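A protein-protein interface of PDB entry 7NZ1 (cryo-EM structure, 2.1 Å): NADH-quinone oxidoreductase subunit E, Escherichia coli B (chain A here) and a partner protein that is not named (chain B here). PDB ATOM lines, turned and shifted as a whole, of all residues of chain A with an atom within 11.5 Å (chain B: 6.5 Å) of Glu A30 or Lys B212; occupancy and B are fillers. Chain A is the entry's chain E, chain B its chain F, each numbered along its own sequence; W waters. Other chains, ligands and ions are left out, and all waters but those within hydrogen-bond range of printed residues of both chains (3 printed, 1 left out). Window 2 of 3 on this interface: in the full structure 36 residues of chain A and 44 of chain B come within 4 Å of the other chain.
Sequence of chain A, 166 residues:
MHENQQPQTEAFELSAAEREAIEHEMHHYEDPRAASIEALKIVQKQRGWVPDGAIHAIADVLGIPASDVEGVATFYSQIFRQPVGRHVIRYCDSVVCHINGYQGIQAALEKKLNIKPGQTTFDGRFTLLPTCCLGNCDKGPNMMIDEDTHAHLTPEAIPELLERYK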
ATOM      1  N   GLU A  23      -6.970 -12.973 -12.672  1.00  0.00           N
ATOM      2  CA  GLU A  23      -7.504 -11.623 -12.794  1.00  0.00           C
ATOM      3  C   GLU A  23      -7.477 -11.109 -14.228  1.00  0.00           C
ATOM      4  O   GLU A  23      -8.196 -10.155 -14.536  1.00  0.00           O
ATOM      5  CB  GLU A  23      -6.732 -10.679 -11.875  1.00  0.00           C
ATOM      6  CG  GLU A  23      -7.048 -10.888 -10.400  1.00  0.00           C
ATOM      7  CD  GLU A  23      -5.978 -10.330  -9.488  1.00  0.00           C
ATOM      8  OE1 GLU A  23      -4.792 -10.363  -9.874  1.00  0.00           O
ATOM      9  OE2 GLU A  23      -6.321  -9.848  -8.387  1.00  0.00           O
ATOM     10  N   HIS A  24      -6.673 -11.719 -15.102  1.00  0.00           N
ATOM     11  CA  HIS A  24      -6.711 -11.386 -16.522  1.00  0.00           C
ATOM     12  C   HIS A  24      -8.039 -11.789 -17.155  1.00  0.00           C
ATOM     13  O   HIS A  24      -8.592 -11.046 -17.973  1.00  0.00           O
ATOM     14  CB  HIS A  24      -5.541 -12.055 -17.245  1.00  0.00           C
ATOM     15  CG  HIS A  24      -5.482 -11.757 -18.708  1.00  0.00           C
ATOM     16  ND1 HIS A  24      -5.827 -10.532 -19.236  1.00  0.00           N
ATOM     17  CD2 HIS A  24      -5.103 -12.525 -19.758  1.00  0.00           C
ATOM     18  CE1 HIS A  24      -5.673 -10.561 -20.548  1.00  0.00           C
ATOM     19  NE2 HIS A  24      -5.230 -11.757 -20.889  1.00  0.00           N
ATOM     20  N   GLU A  25      -8.572 -12.952 -16.786  1.00  0.00           N
ATOM     21  CA  GLU A  25      -9.820 -13.426 -17.368  1.00  0.00           C
ATOM     22  C   GLU A  25     -11.070 -12.920 -16.660  1.00  0.00           C
ATOM     23  O   GLU A  25     -12.173 -13.182 -17.143  1.00  0.00           O
ATOM     24  CB  GLU A  25      -9.837 -14.955 -17.418  1.00  0.00           C
ATOM     25  CG  GLU A  25      -8.984 -15.506 -18.548  1.00  0.00           C
ATOM     26  CD  GLU A  25      -9.654 -16.641 -19.288  1.00  0.00           C
ATOM     27  OE1 GLU A  25     -10.890 -16.776 -19.182  1.00  0.00           O
ATOM     28  OE2 GLU A  25      -8.944 -17.407 -19.975  1.00  0.00           O
ATOM     29  N   MET A  26     -10.939 -12.201 -15.540  1.00  0.00           N
ATOM     30  CA  MET A  26     -12.110 -11.569 -14.939  1.00  0.00           C
ATOM     31  C   MET A  26     -12.563 -10.345 -15.722  1.00  0.00           C
ATOM     32  O   MET A  26     -13.705  -9.907 -15.558  1.00  0.00           O
ATOM     33  CB  MET A  26     -11.827 -11.181 -13.489  1.00  0.00           C
ATOM     34  CG  MET A  26     -11.510 -12.364 -12.584  1.00  0.00           C
ATOM     35  SD  MET A  26     -11.356 -11.995 -10.822  1.00  0.00           S
ATOM     36  CE  MET A  26     -11.290 -10.210 -10.772  1.00  0.00           C
ATOM     37  N   HIS A  27     -11.698  -9.793 -16.572  1.00  0.00           N
ATOM     38  CA  HIS A  27     -12.060  -8.655 -17.403  1.00  0.00           C
ATOM     39  C   HIS A  27     -13.012  -9.031 -18.531  1.00  0.00           C
ATOM     40  O   HIS A  27     -13.694  -8.152 -19.066  1.00  0.00           O
ATOM     41  CB  HIS A  27     -10.803  -8.010 -17.992  1.00  0.00           C
ATOM     42  CG  HIS A  27      -9.957  -7.292 -16.986  1.00  0.00           C
ATOM     43  ND1 HIS A  27     -10.221  -6.003 -16.580  1.00  0.00           N
ATOM     44  CD2 HIS A  27      -8.843  -7.675 -16.319  1.00  0.00           C
ATOM     45  CE1 HIS A  27      -9.311  -5.624 -15.701  1.00  0.00           C
ATOM     46  NE2 HIS A  27      -8.461  -6.620 -15.528  1.00  0.00           N
ATOM     47  N   HIS A  28     -13.086 -10.311 -18.897  1.00  0.00           N
ATOM     48  CA  HIS A  28     -13.810 -10.747 -20.081  1.00  0.00           C
ATOM     49  C   HIS A  28     -15.250 -11.158 -19.781  1.00  0.00           C
ATOM     50  O   HIS A  28     -15.885 -11.794 -20.626  1.00  0.00           O
ATOM     51  CB  HIS A  28     -13.068 -11.907 -20.752  1.00  0.00           C
ATOM     52  CG  HIS A  28     -11.589 -11.702 -20.863  1.00  0.00           C
ATOM     53  ND1 HIS A  28     -10.681 -12.711 -20.630  1.00  0.00           N
ATOM     54  CD2 HIS A  28     -10.860 -10.603 -21.172  1.00  0.00           C
ATOM     55  CE1 HIS A  28      -9.456 -12.247 -20.802  1.00  0.00           C
ATOM     56  NE2 HIS A  28      -9.538 -10.971 -21.130  1.00  0.00           N
ATOM     57  N   TYR A  29     -15.778 -10.798 -18.612  1.00  0.00           N
ATOM     58  CA  TYR A  29     -17.119 -11.196 -18.200  1.00  0.00           C
ATOM     59  C   TYR A  29     -17.761 -10.077 -17.388  1.00  0.00           C
ATOM     60  O   TYR A  29     -17.078  -9.193 -16.868  1.00  0.00           O
ATOM     61  CB  TYR A  29     -17.108 -12.478 -17.356  1.00  0.00           C
ATOM     62  CG  TYR A  29     -16.420 -13.682 -17.963  1.00  0.00           C
ATOM     63  CD1 TYR A  29     -16.987 -14.372 -19.028  1.00  0.00           C
ATOM     64  CD2 TYR A  29     -15.224 -14.151 -17.437  1.00  0.00           C
ATOM     65  CE1 TYR A  29     -16.365 -15.482 -19.569  1.00  0.00           C
ATOM     66  CE2 TYR A  29     -14.596 -15.257 -17.968  1.00  0.00           C
ATOM     67  CZ  TYR A  29     -15.169 -15.918 -19.029  1.00  0.00           C
ATOM     68  OH  TYR A  29     -14.535 -17.019 -19.547  1.00  0.00           O
ATOM     69  N   GLU A  30     -19.096 -10.120 -17.308  1.00  0.00           N
ATOM     70  CA  GLU A  30     -19.836  -9.243 -16.400  1.00  0.00           C
ATOM     71  C   GLU A  30     -19.525  -9.538 -14.936  1.00  0.00           C
ATOM     72  O   GLU A  30     -19.376  -8.615 -14.128  1.00  0.00           O
ATOM     73  CB  GLU A  30     -21.338  -9.400 -16.620  1.00  0.00           C
ATOM     74  CG  GLU A  30     -21.891  -8.806 -17.876  1.00  0.00           C
ATOM     75  CD  GLU A  30     -23.372  -8.499 -17.751  1.00  0.00           C
ATOM     76  OE1 GLU A  30     -23.916  -8.667 -16.643  1.00  0.00           O
ATOM     77  OE2 GLU A  30     -23.995  -8.103 -18.756  1.00  0.00           O
ATOM     78  N   ASP A  31     -19.447 -10.818 -14.574  1.00  0.00           N
ATOM     79  CA  ASP A  31     -19.312 -11.345 -13.227  1.00  0.00           C
ATOM     80  C   ASP A  31     -17.968 -12.051 -13.070  1.00  0.00           C
ATOM     81  O   ASP A  31     -17.537 -12.750 -13.991  1.00  0.00           O
ATOM     82  CB  ASP A  31     -20.463 -12.338 -12.971  1.00  0.00           C
ATOM     83  CG  ASP A  31     -20.935 -12.378 -11.523  1.00  0.00           C
ATOM     84  OD1 ASP A  31     -20.138 -12.170 -10.594  1.00  0.00           O
ATOM     85  OD2 ASP A  31     -22.142 -12.626 -11.310  1.00  0.00           O
ATOM     86  N   PRO A  32     -17.277 -11.904 -11.931  1.00  0.00           N
ATOM     87  CA  PRO A  32     -16.094 -12.743 -11.675  1.00  0.00           C
ATOM     88  C   PRO A  32     -16.397 -14.210 -11.398  1.00  0.00           C
ATOM     89  O   PRO A  32     -15.449 -15.006 -11.365  1.00  0.00           O
ATOM     90  CB  PRO A  32     -15.441 -12.066 -10.459  1.00  0.00           C
ATOM     91  CG  PRO A  32     -16.517 -11.270  -9.846  1.00  0.00           C
ATOM     92  CD  PRO A  32     -17.290 -10.748 -11.021  1.00  0.00           C
ATOM     93  N   ARG A  33     -17.661 -14.579 -11.158  1.00  0.00           N
ATOM     94  CA  ARG A  33     -18.034 -15.983 -10.991  1.00  0.00           C
ATOM     95  C   ARG A  33     -17.757 -16.785 -12.258  1.00  0.00           C
ATOM     96  O   ARG A  33     -17.397 -17.963 -12.183  1.00  0.00           O
ATOM     97  CB  ARG A  33     -19.514 -16.086 -10.608  1.00  0.00           C
ATOM     98  CG  ARG A  33     -20.039 -17.502 -10.366  1.00  0.00           C
ATOM     99  CD  ARG A  33     -21.534 -17.515 -10.116  1.00  0.00           C
ATOM    100  NE  ARG A  33     -21.872 -16.948  -8.817  1.00  0.00           N
ATOM    101  CZ  ARG A  33     -21.913 -17.632  -7.684  1.00  0.00           C
ATOM    102  NH1 ARG A  33     -21.659 -18.929  -7.647  1.00  0.00           N
ATOM    103  NH2 ARG A  33     -22.214 -16.995  -6.557  1.00  0.00           N
ATOM    104  N   ALA A  34     -17.907 -16.152 -13.425  1.00  0.00           N
ATOM    105  CA  ALA A  34     -17.682 -16.797 -14.714  1.00  0.00           C
ATOM    106  C   ALA A  34     -16.238 -17.250 -14.936  1.00  0.00           C
ATOM    107  O   ALA A  34     -16.001 -18.111 -15.786  1.00  0.00           O
ATOM    108  CB  ALA A  34     -18.116 -15.859 -15.830  1.00  0.00           C
ATOM    109  N   ALA A  35     -15.272 -16.684 -14.217  1.00  0.00           N
ATOM    110  CA  ALA A  35     -13.875 -17.070 -14.371  1.00  0.00           C
ATOM    111  C   ALA A  35     -13.494 -18.296 -13.549  1.00  0.00           C
ATOM    112  O   ALA A  35     -12.317 -18.667 -13.549  1.00  0.00           O
ATOM    113  CB  ALA A  35     -12.962 -15.905 -13.989  1.00  0.00           C
ATOM    114  N   SER A  36     -14.451 -18.900 -12.833  1.00  0.00           N
ATOM    115  CA  SER A  36     -14.155 -19.987 -11.901  1.00  0.00           C
ATOM    116  C   SER A  36     -13.614 -21.241 -12.585  1.00  0.00           C
ATOM    117  O   SER A  36     -12.712 -21.887 -12.044  1.00  0.00           O
ATOM    118  CB  SER A  36     -15.392 -20.305 -11.065  1.00  0.00           C
ATOM    119  OG  SER A  36     -15.385 -21.648 -10.622  1.00  0.00           O
ATOM    120  N   LEU A  62     -12.001 -14.500  -6.507  1.00  0.00           N
ATOM    121  CA  LEU A  62     -13.191 -14.258  -7.313  1.00  0.00           C
ATOM    122  C   LEU A  62     -14.337 -13.599  -6.550  1.00  0.00           C
ATOM    123  O   LEU A  62     -15.241 -13.052  -7.185  1.00  0.00           O
ATOM    124  CB  LEU A  62     -13.687 -15.574  -7.900  1.00  0.00           C
ATOM    125  CG  LEU A  62     -12.709 -16.285  -8.822  1.00  0.00           C
ATOM    126  CD1 LEU A  62     -13.358 -17.532  -9.299  1.00  0.00           C
ATOM    127  CD2 LEU A  62     -12.349 -15.406  -9.992  1.00  0.00           C
ATOM    128  N   GLY A  63     -14.320 -13.626  -5.220  1.00  0.00           N
ATOM    129  CA  GLY A  63     -15.430 -13.088  -4.449  1.00  0.00           C
ATOM    130  C   GLY A  63     -16.696 -13.920  -4.467  1.00  0.00           C
ATOM    131  O   GLY A  63     -17.797 -13.364  -4.422  1.00  0.00           O
ATOM    132  N   ILE A  64     -16.569 -15.237  -4.540  1.00  0.00           N
ATOM    133  CA  ILE A  64     -17.697 -16.162  -4.462  1.00  0.00           C
ATOM    134  C   ILE A  64     -17.384 -17.140  -3.337  1.00  0.00           C
ATOM    135  O   ILE A  64     -16.213 -17.271  -2.944  1.00  0.00           O
ATOM    136  CB  ILE A  64     -17.956 -16.862  -5.818  1.00  0.00           C
ATOM    137  CG1 ILE A  64     -16.668 -17.412  -6.417  1.00  0.00           C
ATOM    138  CG2 ILE A  64     -18.652 -15.920  -6.791  1.00  0.00           C
ATOM    139  CD1 ILE A  64     -16.917 -18.459  -7.448  1.00  0.00           C
ATOM    140  N   MET B  82     -33.017  -2.766 -23.825  1.00  0.00           N
ATOM    141  CA  MET B  82     -32.225  -3.988 -23.719  1.00  0.00           C
ATOM    142  C   MET B  82     -31.034  -3.860 -24.669  1.00  0.00           C
ATOM    143  O   MET B  82     -31.002  -4.422 -25.764  1.00  0.00           O
ATOM    144  CB  MET B  82     -33.090  -5.199 -24.045  1.00  0.00           C
ATOM    145  CG  MET B  82     -34.309  -5.316 -23.137  1.00  0.00           C
ATOM    146  SD  MET B  82     -34.844  -6.991 -22.796  1.00  0.00           S
ATOM    147  CE  MET B  82     -33.711  -7.372 -21.468  1.00  0.00           C
ATOM    148  N   ILE B  84     -27.669  -4.638 -23.905  1.00  0.00           N
ATOM    149  CA  ILE B  84     -26.617  -5.639 -23.743  1.00  0.00           C
ATOM    150  C   ILE B  84     -27.154  -6.983 -24.223  1.00  0.00           C
ATOM    151  O   ILE B  84     -28.061  -7.559 -23.615  1.00  0.00           O
ATOM    152  CB  ILE B  84     -26.127  -5.715 -22.291  1.00  0.00           C
ATOM    153  CG1 ILE B  84     -25.454  -4.400 -21.894  1.00  0.00           C
ATOM    154  CG2 ILE B  84     -25.175  -6.888 -22.099  1.00  0.00           C
ATOM    155  CD1 ILE B  84     -24.241  -4.073 -22.718  1.00  0.00           C
ATOM    156  N   ARG B  85     -26.593  -7.483 -25.323  1.00  0.00           N
ATOM    157  CA  ARG B  85     -26.999  -8.745 -25.929  1.00  0.00           C
ATOM    158  C   ARG B  85     -25.764  -9.586 -26.215  1.00  0.00           C
ATOM    159  O   ARG B  85     -24.683  -9.054 -26.475  1.00  0.00           O
ATOM    160  CB  ARG B  85     -27.797  -8.521 -27.227  1.00  0.00           C
ATOM    161  CG  ARG B  85     -29.056  -7.694 -27.037  1.00  0.00           C
ATOM    162  CD  ARG B  85     -29.727  -7.315 -28.327  1.00  0.00           C
ATOM    163  NE  ARG B  85     -30.756  -6.313 -28.082  1.00  0.00           N
ATOM    164  CZ  ARG B  85     -32.055  -6.562 -28.019  1.00  0.00           C
ATOM    165  NH1 ARG B  85     -32.538  -7.774 -28.231  1.00  0.00           N
ATOM    166  NH2 ARG B  85     -32.893  -5.569 -27.741  1.00  0.00           N
ATOM    167  N   TYR B  86     -25.928 -10.906 -26.154  1.00  0.00           N
ATOM    168  CA  TYR B  86     -24.825 -11.836 -26.349  1.00  0.00           C
ATOM    169  C   TYR B  86     -25.126 -12.837 -27.453  1.00  0.00           C
ATOM    170  O   TYR B  86     -26.270 -13.253 -27.650  1.00  0.00           O
ATOM    171  CB  TYR B  86     -24.510 -12.598 -25.068  1.00  0.00           C
ATOM    172  CG  TYR B  86     -24.013 -11.700 -23.978  1.00  0.00           C
ATOM    173  CD1 TYR B  86     -22.725 -11.187 -24.019  1.00  0.00           C
ATOM    174  CD2 TYR B  86     -24.832 -11.361 -22.907  1.00  0.00           C
ATOM    175  CE1 TYR B  86     -22.264 -10.363 -23.031  1.00  0.00           C
ATOM    176  CE2 TYR B  86     -24.379 -10.535 -21.909  1.00  0.00           C
ATOM    177  CZ  TYR B  86     -23.093 -10.040 -21.980  1.00  0.00           C
ATOM    178  OH  TYR B  86     -22.628  -9.212 -21.005  1.00  0.00           O
ATOM    179  N   TYR B 126     -23.016  -7.089 -28.622  1.00  0.00           N
ATOM    180  CA  TYR B 126     -21.701  -6.468 -28.493  1.00  0.00           C
ATOM    181  C   TYR B 126     -20.586  -7.474 -28.213  1.00  0.00           C
ATOM    182  O   TYR B 126     -19.429  -7.210 -28.562  1.00  0.00           O
ATOM    183  CB  TYR B 126     -21.744  -5.366 -27.428  1.00  0.00           C
ATOM    184  CG  TYR B 126     -21.482  -5.788 -25.998  1.00  0.00           C
ATOM    185  CD1 TYR B 126     -22.362  -6.626 -25.329  1.00  0.00           C
ATOM    186  CD2 TYR B 126     -20.380  -5.298 -25.300  1.00  0.00           C
ATOM    187  CE1 TYR B 126     -22.136  -6.995 -24.019  1.00  0.00           C
ATOM    188  CE2 TYR B 126     -20.148  -5.657 -23.982  1.00  0.00           C
ATOM    189  CZ  TYR B 126     -21.029  -6.507 -23.348  1.00  0.00           C
ATOM    190  OH  TYR B 126     -20.811  -6.879 -22.043  1.00  0.00           O
ATOM    191  N   ARG B 127     -20.881  -8.601 -27.567  1.00  0.00           N
ATOM    192  CA  ARG B 127     -19.852  -9.569 -27.208  1.00  0.00           C
ATOM    193  C   ARG B 127     -20.217 -10.960 -27.711  1.00  0.00           C
ATOM    194  O   ARG B 127     -21.387 -11.349 -27.703  1.00  0.00           O
ATOM    195  CB  ARG B 127     -19.627  -9.611 -25.692  1.00  0.00           C
ATOM    196  CG  ARG B 127     -18.493  -8.716 -25.222  1.00  0.00           C
ATOM    197  CD  ARG B 127     -18.281  -8.812 -23.728  1.00  0.00           C
ATOM    198  NE  ARG B 127     -17.422  -7.743 -23.238  1.00  0.00           N
ATOM    199  CZ  ARG B 127     -17.055  -7.598 -21.974  1.00  0.00           C
ATOM    200  NH1 ARG B 127     -17.474  -8.429 -21.033  1.00  0.00           N
ATOM    201  NH2 ARG B 127     -16.251  -6.592 -21.644  1.00  0.00           N
ATOM    202  N   TYR B 129     -18.966 -15.169 -27.477  1.00  0.00           N
ATOM    203  CA  TYR B 129     -18.185 -16.203 -26.810  1.00  0.00           C
ATOM    204  C   TYR B 129     -18.264 -17.505 -27.594  1.00  0.00           C
ATOM    205  O   TYR B 129     -19.360 -17.981 -27.904  1.00  0.00           O
ATOM    206  CB  TYR B 129     -18.675 -16.429 -25.377  1.00  0.00           C
ATOM    207  CG  TYR B 129     -18.583 -15.215 -24.487  1.00  0.00           C
ATOM    208  CD1 TYR B 129     -17.410 -14.917 -23.809  1.00  0.00           C
ATOM    209  CD2 TYR B 129     -19.674 -14.371 -24.318  1.00  0.00           C
ATOM    210  CE1 TYR B 129     -17.320 -13.807 -22.988  1.00  0.00           C
ATOM    211  CE2 TYR B 129     -19.596 -13.258 -23.500  1.00  0.00           C
ATOM    212  CZ  TYR B 129     -18.413 -12.981 -22.843  1.00  0.00           C
ATOM    213  OH  TYR B 129     -18.326 -11.883 -22.029  1.00  0.00           O
ATOM    214  N   PRO B 204     -33.923 -18.110 -23.816  1.00  0.00           N
ATOM    215  CA  PRO B 204     -32.700 -17.294 -23.690  1.00  0.00           C
ATOM    216  C   PRO B 204     -32.690 -16.053 -24.560  1.00  0.00           C
ATOM    217  O   PRO B 204     -31.876 -15.158 -24.305  1.00  0.00           O
ATOM    218  CB  PRO B 204     -31.581 -18.263 -24.094  1.00  0.00           C
ATOM    219  CG  PRO B 204     -32.158 -19.605 -23.922  1.00  0.00           C
ATOM    220  CD  PRO B 204     -33.594 -19.473 -24.273  1.00  0.00           C
ATOM    221  N   ALA B 205     -33.535 -16.000 -25.599  1.00  0.00           N
ATOM    222  CA  ALA B 205     -33.725 -14.790 -26.395  1.00  0.00           C
ATOM    223  C   ALA B 205     -34.158 -13.593 -25.553  1.00  0.00           C
ATOM    224  O   ALA B 205     -33.805 -12.458 -25.877  1.00  0.00           O
ATOM    225  CB  ALA B 205     -34.745 -15.056 -27.496  1.00  0.00           C
ATOM    226  N   THR B 206     -34.895 -13.818 -24.465  1.00  0.00           N
ATOM    227  CA  THR B 206     -35.248 -12.750 -23.541  1.00  0.00           C
ATOM    228  C   THR B 206     -34.365 -12.755 -22.298  1.00  0.00           C
ATOM    229  O   THR B 206     -33.802 -11.721 -21.936  1.00  0.00           O
ATOM    230  CB  THR B 206     -36.726 -12.846 -23.138  1.00  0.00           C
ATOM    231  OG1 THR B 206     -36.933 -14.000 -22.317  1.00  0.00           O
ATOM    232  CG2 THR B 206     -37.600 -12.950 -24.376  1.00  0.00           C
ATOM    233  N   SER B 207     -34.228 -13.905 -21.639  1.00  0.00           N
ATOM    234  CA  SER B 207     -33.444 -14.032 -20.411  1.00  0.00           C
ATOM    235  C   SER B 207     -32.401 -15.135 -20.577  1.00  0.00           C
ATOM    236  O   SER B 207     -32.697 -16.315 -20.364  1.00  0.00           O
ATOM    237  CB  SER B 207     -34.357 -14.311 -19.226  1.00  0.00           C
ATOM    238  OG  SER B 207     -35.419 -13.381 -19.171  1.00  0.00           O
ATOM    239  N   GLY B 208     -31.180 -14.752 -20.938  1.00  0.00           N
ATOM    240  CA  GLY B 208     -30.107 -15.707 -21.136  1.00  0.00           C
ATOM    241  C   GLY B 208     -28.919 -15.493 -20.220  1.00  0.00           C
ATOM    242  O   GLY B 208     -29.054 -15.559 -18.996  1.00  0.00           O
ATOM    243  N   ALA B 209     -27.744 -15.278 -20.814  1.00  0.00           N
ATOM    244  CA  ALA B 209     -26.506 -15.112 -20.058  1.00  0.00           C
ATOM    245  C   ALA B 209     -26.530 -13.817 -19.258  1.00  0.00           C
ATOM    246  O   ALA B 209     -26.674 -12.734 -19.833  1.00  0.00           O
ATOM    247  CB  ALA B 209     -25.310 -15.137 -21.003  1.00  0.00           C
ATOM    248  N   TRP B 210     -26.375 -13.952 -17.934  1.00  0.00           N
ATOM    249  CA  TRP B 210     -26.419 -12.856 -16.956  1.00  0.00           C
ATOM    250  C   TRP B 210     -27.712 -12.048 -17.063  1.00  0.00           C
ATOM    251  O   TRP B 210     -27.719 -10.827 -16.907  1.00  0.00           O
ATOM    252  CB  TRP B 210     -25.178 -11.964 -17.061  1.00  0.00           C
ATOM    253  CG  TRP B 210     -23.908 -12.744 -16.928  1.00  0.00           C
ATOM    254  CD1 TRP B 210     -23.391 -13.272 -15.784  1.00  0.00           C
ATOM    255  CD2 TRP B 210     -22.996 -13.088 -17.974  1.00  0.00           C
ATOM    256  NE1 TRP B 210     -22.214 -13.924 -16.050  1.00  0.00           N
ATOM    257  CE2 TRP B 210     -21.948 -13.824 -17.389  1.00  0.00           C
ATOM    258  CE3 TRP B 210     -22.961 -12.842 -19.349  1.00  0.00           C
ATOM    259  CZ2 TRP B 210     -20.879 -14.321 -18.132  1.00  0.00           C
ATOM    260  CZ3 TRP B 210     -21.902 -13.334 -20.084  1.00  0.00           C
ATOM    261  CH2 TRP B 210     -20.877 -14.066 -19.475  1.00  0.00           C
ATOM    262  N   GLY B 211     -28.814 -12.757 -17.320  1.00  0.00           N
ATOM    263  CA  GLY B 211     -30.127 -12.158 -17.497  1.00  0.00           C
ATOM    264  C   GLY B 211     -30.218 -11.178 -18.642  1.00  0.00           C
ATOM    265  O   GLY B 211     -30.969 -10.207 -18.558  1.00  0.00           O
ATOM    266  N   LYS B 212     -29.484 -11.417 -19.716  1.00  0.00           N
ATOM    267  CA  LYS B 212     -29.452 -10.560 -20.885  1.00  0.00           C
ATOM    268  C   LYS B 212     -29.973 -11.360 -22.068  1.00  0.00           C
ATOM    269  O   LYS B 212     -29.989 -12.594 -22.019  1.00  0.00           O
ATOM    270  CB  LYS B 212     -28.025 -10.061 -21.160  1.00  0.00           C
ATOM    271  CG  LYS B 212     -27.414  -9.311 -19.999  1.00  0.00           C
ATOM    272  CD  LYS B 212     -28.206  -8.072 -19.660  1.00  0.00           C
ATOM    273  CE  LYS B 212     -27.429  -7.179 -18.715  1.00  0.00           C
ATOM    274  NZ  LYS B 212     -27.087  -7.886 -17.452  1.00  0.00           N
ATOM    275  N   PRO B 213     -30.496 -10.697 -23.098  1.00  0.00           N
ATOM    276  CA  PRO B 213     -30.887 -11.413 -24.321  1.00  0.00           C
ATOM    277  C   PRO B 213     -29.713 -12.141 -24.972  1.00  0.00           C
ATOM    278  O   PRO B 213     -28.648 -11.567 -25.195  1.00  0.00           O
ATOM    279  CB  PRO B 213     -31.429 -10.290 -25.205  1.00  0.00           C
ATOM    280  CG  PRO B 213     -31.925  -9.292 -24.264  1.00  0.00           C
ATOM    281  CD  PRO B 213     -30.972  -9.303 -23.125  1.00  0.00           C
ATOM    282  N   THR B 214     -29.923 -13.420 -25.268  1.00  0.00           N
ATOM    283  CA  THR B 214     -28.844 -14.300 -25.705  1.00  0.00           C
ATOM    284  C   THR B 214     -29.306 -15.244 -26.824  1.00  0.00           C
ATOM    285  O   THR B 214     -30.419 -15.754 -26.784  1.00  0.00           O
ATOM    286  CB  THR B 214     -28.315 -15.145 -24.507  1.00  0.00           C
ATOM    287  OG1 THR B 214     -28.049 -14.293 -23.389  1.00  0.00           O
ATOM    288  CG2 THR B 214     -27.044 -15.860 -24.854  1.00  0.00           C
HETATM  289  O   HOH W   1     -20.252 -10.442 -20.314  1.00  0.00           O
HETATM  290  O   HOH W   2     -26.262  -9.033 -15.266  1.00  0.00           O
HETATM  291  O   HOH W   3     -17.742  -7.017 -18.451  1.00  0.00           O
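Among the printed residues, merely in contact across the chains: Glu A30 with Trp B210 (3.6 Å), His A28 with Arg B127 (3.7 Å), Glu A30 with Ile B84 (3.7 Å), Tyr A29 with Arg B127 (3.8 Å), Asp A31 with Trp B210 (3.9 Å), Ala A34 with Trp B210 (3.9 Å), Tyr A29 with Tyr B129 (3.9 Å), Tyr A29 with Trp B210 (3.9 Å) and His A27 with Arg B127 (3.95 Å).
Printed residues of chain B that touch a printed residue of chain A: Ile B84, Tyr B86, Arg B127, Tyr B129, Trp B210 and Lys B212.
Printed residues of chain A that touch a printed residue of chain B: His A27, His A28, Tyr A29, Glu A30, Asp A31 and Ala A34.
Among the printed residues, 12 pairs touch across the chains.
Among the printed residues, Asp or Glu carboxylates within 4 Å of a Lys or Arg side-chain nitrogen of the other chain: Glu A30 with Lys B212 (3.4 Å).
The backbone carbonyl oxygen (O) of His A24 sits close to a ring nitrogen (NE2) of His A28 (3.3 Å).
OH of Tyr B86 lies within hydrogen-bond range of OH of Tyr B126.
O of Pro B213 lies within hydrogen-bond range of N of Tyr B86 (3.0 Å).
O of Trp B210 is in hydrogen-bond range of NZ of Lys B212, at 3.1 Å.
OG1 of Thr B214 is in hydrogen-bond range of O of Lys B212 (2.9 Å).
Of the printed residues of chain B, Glu A30 touches Ile B84 (3.7 Å), Tyr B86 (2.9 Å), Trp B210 (3.6 Å) and Lys B212 (3.4 Å).
Lys B212 touches one residue of chain A.
Of chain A, only Glu A30 (3.7 Å) comes within 4 Å of Ile B84.
Of the printed residues of chain A, Tyr B86 touches Glu A30 (2.9 Å).
No residue of chain A comes within 4 Å of Ser B207.
No residue of chain A comes within 4 Å of Gly B208.
No residue of chain A comes within 4 Å of Gly B211.
No residue of chain A comes within 4 Å of Thr B214.
Printed residues of chain A within 4 Å of Arg B127: His A27 (3.95 Å), His A28 (3.7 Å) and Tyr A29 (3.8 Å).
Printed residues of chain A within 4 Å of Tyr B129: His A28 (2.8 Å) and Tyr A29 (3.9 Å).
Of the printed residues of chain B, His A28 touches Arg B127 and Tyr B129.
Of the printed residues of chain B, Asp A31 touches Trp B210 (3.9 Å).
Of the printed residues of chain B, His A27 touches Arg B127.
The backbone carbonyl oxygen of His A28 is in hydrogen-bond range of the side-chain hydroxyl of Tyr B129, 2.8 Å away.
OE2 of Glu A30 sits at hydrogen-bond distance from OH of Tyr B86, 2.9 Å away.
NZ of Lys B212 is in salt-bridge range of OE2 of Glu A30 (3.4 Å).
Water W2 lies within hydrogen-bond range of the side-chain amino group (NZ) of Lys B212 (2.6 Å), the side-chain carboxylate (OE1) of Glu A30 (2.7 Å) and the backbone carbonyl oxygen (O) of Trp B210 (2.8 Å).
Water W1 lies within hydrogen-bond range of the side-chain hydroxyl (OH) of Tyr B86 (2.8 Å), the side-chain hydroxyl (OH) of Tyr B129 (3.0 Å) and the backbone NH (N) of Glu A30 (3.2 Å).
Water W3 bridges O of Tyr A29 (2.8 Å) and NH1 of Arg B127 (3.0 Å).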
